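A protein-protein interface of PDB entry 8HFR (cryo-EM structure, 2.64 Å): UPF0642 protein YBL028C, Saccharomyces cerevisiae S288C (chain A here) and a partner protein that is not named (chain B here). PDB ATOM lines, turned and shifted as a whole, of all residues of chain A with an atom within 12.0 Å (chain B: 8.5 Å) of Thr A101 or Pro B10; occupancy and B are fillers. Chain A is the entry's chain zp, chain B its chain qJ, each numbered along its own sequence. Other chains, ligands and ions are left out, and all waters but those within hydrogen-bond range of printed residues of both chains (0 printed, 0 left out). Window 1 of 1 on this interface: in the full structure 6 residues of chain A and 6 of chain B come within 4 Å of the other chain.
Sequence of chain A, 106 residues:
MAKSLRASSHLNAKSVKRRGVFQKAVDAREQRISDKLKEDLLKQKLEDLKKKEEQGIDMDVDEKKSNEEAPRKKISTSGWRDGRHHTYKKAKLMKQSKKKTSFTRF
Thr A101 touches two residues of chain B.
Of chain B, only Arg B9 comes within 4 Å of Ser A102.
No residue of chain A comes within 4 Å of Pro B2.
Of chain A, only Thr A101 (3.2 Å), Ser A102 (3.98 Å) and Phe A103 (3.3 Å) come within 4 Å of Arg B9.
Lys B11 touches none of the printed residues of chain A.
Ser B14 touches just these residues of chain A: Lys A99 and Lys A100.
Printed residues of chain A within 4 Å of Ser B6: Phe A103 (3.7 Å).
Of the printed residues of chain B, Phe A103 touches Ser B6 (3.7 Å), Asn B8 (3.6 Å) and Arg B9 (3.3 Å).
Printed residues of chain B within 4 Å of Lys A99: Ser B14.
Of the printed residues of chain A, Asn B8 touches Phe A103.
The nearest residue of chain A that does not touch Pro B10 is Ser A102 (4.6 Å).
Of the 15 printed residues of chain A, 5 touch a printed residue of chain B.
Hydrophobic or aromatic side chains of chain A that line the printed part of chain B: Phe A103.
Hydrophobic or aromatic side chains of chain B that line the printed part of chain A: Pro B10.
Among the printed residues, no Asp or Glu carboxylate lies within 4 Å of a Lys or Arg side-chain nitrogen of the other chain.
The backbone carbonyl oxygen of Lys A99 sits at hydrogen-bond distance from the side-chain hydroxyl of Ser B14, 3.0 Å away.
The backbone carbonyl oxygen (O) of Lys A100 sits close to the side-chain hydroxyl (OG) of Ser B14 (2.2 Å).
Among the printed residues, merely in contact across the chains: Thr A101 with Arg B9 (3.2 Å), Phe A103 with Arg B9 (3.3 Å), Lys A100 with Pro B10 (3.5 Å), Phe A103 with Asn B8 (3.6 Å), Phe A103 with Ser B6 (3.7 Å), Thr A101 with Pro B10 (3.8 Å) and Ser A102 with Arg B9 (3.98 Å).
O of Pro B10 is in hydrogen-bond range of OG of Ser B14 (3.2 Å).
The backbone NH of Thr A101 lies close to the backbone carbonyl oxygen of Gln A96, at 3.4 Å.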
ATOM      1  N   LYS A  92      -4.604 -17.075 -31.650  1.00  0.00           N
ATOM      2  CA  LYS A  92      -4.684 -17.684 -30.330  1.00  0.00           C
ATOM      3  C   LYS A  92      -5.172 -19.121 -30.418  1.00  0.00           C
ATOM      4  O   LYS A  92      -4.374 -20.054 -30.248  1.00  0.00           O
ATOM      5  CB  LYS A  92      -5.622 -16.880 -29.429  1.00  0.00           C
ATOM      6  N   LEU A  93      -6.462 -19.302 -30.706  1.00  0.00           N
ATOM      7  CA  LEU A  93      -7.120 -20.587 -30.974  1.00  0.00           C
ATOM      8  C   LEU A  93      -6.914 -21.710 -29.956  1.00  0.00           C
ATOM      9  O   LEU A  93      -7.283 -22.854 -30.239  1.00  0.00           O
ATOM     10  CB  LEU A  93      -6.684 -21.110 -32.340  1.00  0.00           C
ATOM     11  N   MET A  94      -6.332 -21.428 -28.789  1.00  0.00           N
ATOM     12  CA  MET A  94      -6.034 -22.476 -27.823  1.00  0.00           C
ATOM     13  C   MET A  94      -6.330 -22.098 -26.380  1.00  0.00           C
ATOM     14  O   MET A  94      -6.323 -22.989 -25.522  1.00  0.00           O
ATOM     15  CB  MET A  94      -4.558 -22.919 -27.921  1.00  0.00           C
ATOM     16  CG  MET A  94      -4.229 -23.960 -28.991  1.00  0.00           C
ATOM     17  SD  MET A  94      -3.905 -23.340 -30.653  1.00  0.00           S
ATOM     18  CE  MET A  94      -2.241 -22.689 -30.466  1.00  0.00           C
ATOM     19  N   LYS A  95      -6.568 -20.818 -26.079  1.00  0.00           N
ATOM     20  CA  LYS A  95      -6.649 -20.365 -24.693  1.00  0.00           C
ATOM     21  C   LYS A  95      -7.892 -20.909 -24.006  1.00  0.00           C
ATOM     22  O   LYS A  95      -7.887 -21.160 -22.799  1.00  0.00           O
ATOM     23  CB  LYS A  95      -6.629 -18.836 -24.635  1.00  0.00           C
ATOM     24  N   GLN A  96      -8.947 -21.159 -24.776  1.00  0.00           N
ATOM     25  CA  GLN A  96     -10.191 -21.702 -24.246  1.00  0.00           C
ATOM     26  C   GLN A  96     -10.033 -23.154 -23.795  1.00  0.00           C
ATOM     27  O   GLN A  96     -10.280 -23.478 -22.629  1.00  0.00           O
ATOM     28  CB  GLN A  96     -11.293 -21.567 -25.295  1.00  0.00           C
ATOM     29  CG  GLN A  96     -12.140 -20.313 -25.133  1.00  0.00           C
ATOM     30  CD  GLN A  96     -12.908 -19.944 -26.390  1.00  0.00           C
ATOM     31  OE1 GLN A  96     -13.628 -20.761 -26.955  1.00  0.00           O
ATOM     32  NE2 GLN A  96     -12.763 -18.700 -26.827  1.00  0.00           N
ATOM     33  N   SER A  97      -9.581 -24.035 -24.688  1.00  0.00           N
ATOM     34  CA  SER A  97      -9.385 -25.425 -24.286  1.00  0.00           C
ATOM     35  C   SER A  97      -8.138 -25.617 -23.431  1.00  0.00           C
ATOM     36  O   SER A  97      -7.915 -26.719 -22.916  1.00  0.00           O
ATOM     37  CB  SER A  97      -9.316 -26.334 -25.514  1.00  0.00           C
ATOM     38  OG  SER A  97     -10.586 -26.454 -26.133  1.00  0.00           O
ATOM     39  N   LYS A  98      -7.311 -24.582 -23.276  1.00  0.00           N
ATOM     40  CA  LYS A  98      -6.231 -24.613 -22.301  1.00  0.00           C
ATOM     41  C   LYS A  98      -6.688 -24.156 -20.921  1.00  0.00           C
ATOM     42  O   LYS A  98      -6.153 -24.617 -19.909  1.00  0.00           O
ATOM     43  CB  LYS A  98      -5.071 -23.742 -22.782  1.00  0.00           C
ATOM     44  N   LYS A  99      -7.677 -23.260 -20.861  1.00  0.00           N
ATOM     45  CA  LYS A  99      -8.194 -22.734 -19.607  1.00  0.00           C
ATOM     46  C   LYS A  99      -9.499 -23.397 -19.175  1.00  0.00           C
ATOM     47  O   LYS A  99     -10.127 -22.912 -18.227  1.00  0.00           O
ATOM     48  CB  LYS A  99      -8.387 -21.219 -19.715  1.00  0.00           C
ATOM     49  N   LYS A 100      -9.918 -24.467 -19.868  1.00  0.00           N
ATOM     50  CA  LYS A 100     -10.990 -25.380 -19.426  1.00  0.00           C
ATOM     51  C   LYS A 100     -12.335 -24.668 -19.291  1.00  0.00           C
ATOM     52  O   LYS A 100     -12.944 -24.631 -18.222  1.00  0.00           O
ATOM     53  CB  LYS A 100     -10.616 -26.087 -18.120  1.00  0.00           C
ATOM     54  N   THR A 101     -12.813 -24.139 -20.411  1.00  0.00           N
ATOM     55  CA  THR A 101     -13.940 -23.220 -20.520  1.00  0.00           C
ATOM     56  C   THR A 101     -14.617 -23.513 -21.854  1.00  0.00           C
ATOM     57  O   THR A 101     -14.703 -24.692 -22.216  1.00  0.00           O
ATOM     58  CB  THR A 101     -13.489 -21.765 -20.346  1.00  0.00           C
ATOM     59  OG1 THR A 101     -14.577 -20.884 -20.628  1.00  0.00           O
ATOM     60  CG2 THR A 101     -12.308 -21.417 -21.203  1.00  0.00           C
ATOM     61  N   SER A 102     -15.210 -22.500 -22.507  1.00  0.00           N
ATOM     62  CA  SER A 102     -15.664 -22.605 -23.899  1.00  0.00           C
ATOM     63  C   SER A 102     -16.857 -23.505 -24.158  1.00  0.00           C
ATOM     64  O   SER A 102     -16.666 -24.706 -24.363  1.00  0.00           O
ATOM     65  CB  SER A 102     -14.544 -23.062 -24.839  1.00  0.00           C
ATOM     66  N   PHE A 103     -18.069 -22.941 -24.045  1.00  0.00           N
ATOM     67  CA  PHE A 103     -19.351 -23.499 -24.484  1.00  0.00           C
ATOM     68  C   PHE A 103     -19.211 -24.336 -25.759  1.00  0.00           C
ATOM     69  O   PHE A 103     -18.465 -23.989 -26.680  1.00  0.00           O
ATOM     70  CB  PHE A 103     -20.363 -22.406 -24.847  1.00  0.00           C
ATOM     71  CG  PHE A 103     -20.426 -21.233 -23.916  1.00  0.00           C
ATOM     72  CD1 PHE A 103     -21.167 -21.280 -22.755  1.00  0.00           C
ATOM     73  CD2 PHE A 103     -19.792 -20.048 -24.248  1.00  0.00           C
ATOM     74  CE1 PHE A 103     -21.248 -20.172 -21.925  1.00  0.00           C
ATOM     75  CE2 PHE A 103     -19.863 -18.944 -23.421  1.00  0.00           C
ATOM     76  CZ  PHE A 103     -20.592 -19.007 -22.259  1.00  0.00           C
ATOM     77  N   THR A 104     -19.929 -25.461 -25.777  1.00  0.00           N
ATOM     78  CA  THR A 104     -20.078 -26.512 -26.787  1.00  0.00           C
ATOM     79  C   THR A 104     -18.893 -27.474 -26.851  1.00  0.00           C
ATOM     80  O   THR A 104     -18.984 -28.469 -27.559  1.00  0.00           O
ATOM     81  CB  THR A 104     -20.350 -25.996 -28.220  1.00  0.00           C
ATOM     82  OG1 THR A 104     -19.191 -25.325 -28.719  1.00  0.00           O
ATOM     83  CG2 THR A 104     -21.533 -25.054 -28.266  1.00  0.00           C
ATOM     84  N   ARG A 105     -17.799 -27.241 -26.131  1.00  0.00           N
ATOM     85  CA  ARG A 105     -16.691 -28.186 -26.155  1.00  0.00           C
ATOM     86  C   ARG A 105     -16.189 -28.414 -24.743  1.00  0.00           C
ATOM     87  O   ARG A 105     -16.340 -27.559 -23.868  1.00  0.00           O
ATOM     88  CB  ARG A 105     -15.553 -27.707 -27.058  1.00  0.00           C
ATOM     89  CG  ARG A 105     -15.847 -27.897 -28.534  1.00  0.00           C
ATOM     90  CD  ARG A 105     -14.998 -27.011 -29.408  1.00  0.00           C
ATOM     91  NE  ARG A 105     -15.681 -26.718 -30.661  1.00  0.00           N
ATOM     92  CZ  ARG A 105     -15.517 -27.408 -31.783  1.00  0.00           C
ATOM     93  NH1 ARG A 105     -14.681 -28.435 -31.817  1.00  0.00           N
ATOM     94  NH2 ARG A 105     -16.187 -27.065 -32.875  1.00  0.00           N
ATOM     95  N   PHE A 106     -15.599 -29.580 -24.525  1.00  0.00           N
ATOM     96  CA  PHE A 106     -15.124 -29.959 -23.201  1.00  0.00           C
ATOM     97  C   PHE A 106     -13.608 -29.821 -23.099  1.00  0.00           C
ATOM     98  O   PHE A 106     -12.981 -29.077 -23.851  1.00  0.00           O
ATOM     99  CB  PHE A 106     -15.544 -31.393 -22.872  1.00  0.00           C
ATOM    100  CG  PHE A 106     -16.914 -31.508 -22.275  1.00  0.00           C
ATOM    101  CD1 PHE A 106     -17.166 -31.059 -20.990  1.00  0.00           C
ATOM    102  CD2 PHE A 106     -17.944 -32.086 -22.987  1.00  0.00           C
ATOM    103  CE1 PHE A 106     -18.425 -31.173 -20.437  1.00  0.00           C
ATOM    104  CE2 PHE A 106     -19.201 -32.209 -22.428  1.00  0.00           C
ATOM    105  CZ  PHE A 106     -19.439 -31.750 -21.155  1.00  0.00           C
ATOM    106  OXT PHE A 106     -12.971 -30.450 -22.256  1.00  0.00           O
ATOM    107  N   PRO B   2     -23.582 -24.264 -12.906  1.00  0.00           N
ATOM    108  CA  PRO B   2     -23.105 -23.182 -12.039  1.00  0.00           C
ATOM    109  C   PRO B   2     -22.948 -21.894 -12.828  1.00  0.00           C
ATOM    110  O   PRO B   2     -22.629 -22.000 -14.012  1.00  0.00           O
ATOM    111  CB  PRO B   2     -21.754 -23.700 -11.539  1.00  0.00           C
ATOM    112  CG  PRO B   2     -21.810 -25.176 -11.755  1.00  0.00           C
ATOM    113  CD  PRO B   2     -22.601 -25.354 -13.000  1.00  0.00           C
ATOM    114  N   SER B   3     -23.153 -20.739 -12.182  1.00  0.00           N
ATOM    115  CA  SER B   3     -23.237 -19.423 -12.827  1.00  0.00           C
ATOM    116  C   SER B   3     -24.377 -19.387 -13.848  1.00  0.00           C
ATOM    117  O   SER B   3     -24.179 -19.555 -15.046  1.00  0.00           O
ATOM    118  CB  SER B   3     -21.917 -18.980 -13.462  1.00  0.00           C
ATOM    119  OG  SER B   3     -21.974 -17.595 -13.750  1.00  0.00           O
ATOM    120  N   SER B   6     -24.522 -18.323 -17.439  1.00  0.00           N
ATOM    121  CA  SER B   6     -23.918 -19.141 -18.492  1.00  0.00           C
ATOM    122  C   SER B   6     -23.750 -20.564 -17.954  1.00  0.00           C
ATOM    123  O   SER B   6     -22.721 -20.888 -17.359  1.00  0.00           O
ATOM    124  CB  SER B   6     -22.590 -18.544 -18.921  1.00  0.00           C
ATOM    125  OG  SER B   6     -21.816 -18.218 -17.786  1.00  0.00           O
ATOM    126  N   ILE B   7     -24.749 -21.416 -18.204  1.00  0.00           N
ATOM    127  CA  ILE B   7     -24.760 -22.744 -17.590  1.00  0.00           C
ATOM    128  C   ILE B   7     -23.920 -23.769 -18.328  1.00  0.00           C
ATOM    129  O   ILE B   7     -23.645 -24.835 -17.771  1.00  0.00           O
ATOM    130  CB  ILE B   7     -26.176 -23.337 -17.467  1.00  0.00           C
ATOM    131  CG1 ILE B   7     -26.910 -23.265 -18.803  1.00  0.00           C
ATOM    132  CG2 ILE B   7     -26.951 -22.633 -16.386  1.00  0.00           C
ATOM    133  CD1 ILE B   7     -27.972 -24.309 -18.964  1.00  0.00           C
ATOM    134  N   ASN B   8     -23.503 -23.491 -19.561  1.00  0.00           N
ATOM    135  CA  ASN B   8     -22.737 -24.447 -20.347  1.00  0.00           C
ATOM    136  C   ASN B   8     -21.242 -24.163 -20.321  1.00  0.00           C
ATOM    137  O   ASN B   8     -20.525 -24.592 -21.225  1.00  0.00           O
ATOM    138  CB  ASN B   8     -23.242 -24.472 -21.789  1.00  0.00           C
ATOM    139  CG  ASN B   8     -24.531 -25.242 -21.941  1.00  0.00           C
ATOM    140  OD1 ASN B   8     -24.835 -26.124 -21.150  1.00  0.00           O
ATOM    141  ND2 ASN B   8     -25.300 -24.905 -22.957  1.00  0.00           N
ATOM    142  N   ARG B   9     -20.753 -23.463 -19.304  1.00  0.00           N
ATOM    143  CA  ARG B   9     -19.344 -23.139 -19.196  1.00  0.00           C
ATOM    144  C   ARG B   9     -18.786 -23.598 -17.853  1.00  0.00           C
ATOM    145  O   ARG B   9     -19.419 -23.368 -16.815  1.00  0.00           O
ATOM    146  CB  ARG B   9     -19.130 -21.638 -19.359  1.00  0.00           C
ATOM    147  CG  ARG B   9     -17.715 -21.262 -19.676  1.00  0.00           C
ATOM    148  CD  ARG B   9     -17.642 -19.905 -20.319  1.00  0.00           C
ATOM    149  NE  ARG B   9     -17.804 -18.830 -19.350  1.00  0.00           N
ATOM    150  CZ  ARG B   9     -18.015 -17.564 -19.683  1.00  0.00           C
ATOM    151  NH1 ARG B   9     -18.081 -17.224 -20.958  1.00  0.00           N
ATOM    152  NH2 ARG B   9     -18.159 -16.643 -18.744  1.00  0.00           N
ATOM    153  N   PRO B  10     -17.629 -24.259 -17.825  1.00  0.00           N
ATOM    154  CA  PRO B  10     -17.048 -24.676 -16.543  1.00  0.00           C
ATOM    155  C   PRO B  10     -16.354 -23.516 -15.845  1.00  0.00           C
ATOM    156  O   PRO B  10     -15.541 -22.807 -16.438  1.00  0.00           O
ATOM    157  CB  PRO B  10     -16.050 -25.768 -16.940  1.00  0.00           C
ATOM    158  CG  PRO B  10     -16.389 -26.115 -18.347  1.00  0.00           C
ATOM    159  CD  PRO B  10     -16.940 -24.886 -18.958  1.00  0.00           C
ATOM    160  N   LYS B  11     -16.672 -23.337 -14.568  1.00  0.00           N
ATOM    161  CA  LYS B  11     -16.204 -22.201 -13.791  1.00  0.00           C
ATOM    162  C   LYS B  11     -15.271 -22.632 -12.667  1.00  0.00           C
ATOM    163  O   LYS B  11     -14.105 -22.207 -12.606  1.00  0.00           O
ATOM    164  CB  LYS B  11     -17.436 -21.479 -13.236  1.00  0.00           C
ATOM    165  CG  LYS B  11     -17.203 -20.139 -12.585  1.00  0.00           C
ATOM    166  CD  LYS B  11     -18.517 -19.624 -12.022  1.00  0.00           C
ATOM    167  CE  LYS B  11     -18.434 -18.183 -11.636  1.00  0.00           C
ATOM    168  NZ  LYS B  11     -18.023 -17.370 -12.800  1.00  0.00           N
ATOM    169  N   LEU B  12     -15.756 -23.524 -11.802  1.00  0.00           N
ATOM    170  CA  LEU B  12     -15.002 -23.939 -10.629  1.00  0.00           C
ATOM    171  C   LEU B  12     -13.795 -24.776 -11.011  1.00  0.00           C
ATOM    172  O   LEU B  12     -12.728 -24.645 -10.400  1.00  0.00           O
ATOM    173  CB  LEU B  12     -15.913 -24.713  -9.682  1.00  0.00           C
ATOM    174  CG  LEU B  12     -15.309 -25.117  -8.340  1.00  0.00           C
ATOM    175  CD1 LEU B  12     -14.795 -23.885  -7.612  1.00  0.00           C
ATOM    176  CD2 LEU B  12     -16.321 -25.862  -7.495  1.00  0.00           C
ATOM    177  N   THR B  13     -13.930 -25.621 -12.033  1.00  0.00           N
ATOM    178  CA  THR B  13     -12.827 -26.497 -12.413  1.00  0.00           C
ATOM    179  C   THR B  13     -11.712 -25.715 -13.091  1.00  0.00           C
ATOM    180  O   THR B  13     -10.529 -26.017 -12.896  1.00  0.00           O
ATOM    181  CB  THR B  13     -13.335 -27.619 -13.315  1.00  0.00           C
ATOM    182  OG1 THR B  13     -13.531 -27.119 -14.642  1.00  0.00           O
ATOM    183  CG2 THR B  13     -14.646 -28.162 -12.785  1.00  0.00           C
ATOM    184  N   SER B  14     -12.071 -24.675 -13.846  1.00  0.00           N
ATOM    185  CA  SER B  14     -11.073 -23.770 -14.404  1.00  0.00           C
ATOM    186  C   SER B  14     -10.341 -23.014 -13.309  1.00  0.00           C
ATOM    187  O   SER B  14      -9.111 -22.847 -13.371  1.00  0.00           O
ATOM    188  CB  SER B  14     -11.743 -22.786 -15.350  1.00  0.00           C
ATOM    189  OG  SER B  14     -12.437 -23.473 -16.364  1.00  0.00           O
ATOM    190  N   ASN B  15     -11.084 -22.559 -12.295  1.00  0.00           N
ATOM    191  CA  ASN B  15     -10.471 -21.855 -11.175  1.00  0.00           C
ATOM    192  C   ASN B  15      -9.503 -22.752 -10.412  1.00  0.00           C
ATOM    193  O   ASN B  15      -8.387 -22.332 -10.083  1.00  0.00           O
ATOM    194  CB  ASN B  15     -11.554 -21.318 -10.248  1.00  0.00           C
ATOM    195  CG  ASN B  15     -12.178 -20.051 -10.771  1.00  0.00           C
ATOM    196  OD1 ASN B  15     -11.662 -19.433 -11.698  1.00  0.00           O
ATOM    197  ND2 ASN B  15     -13.294 -19.656 -10.181  1.00  0.00           N
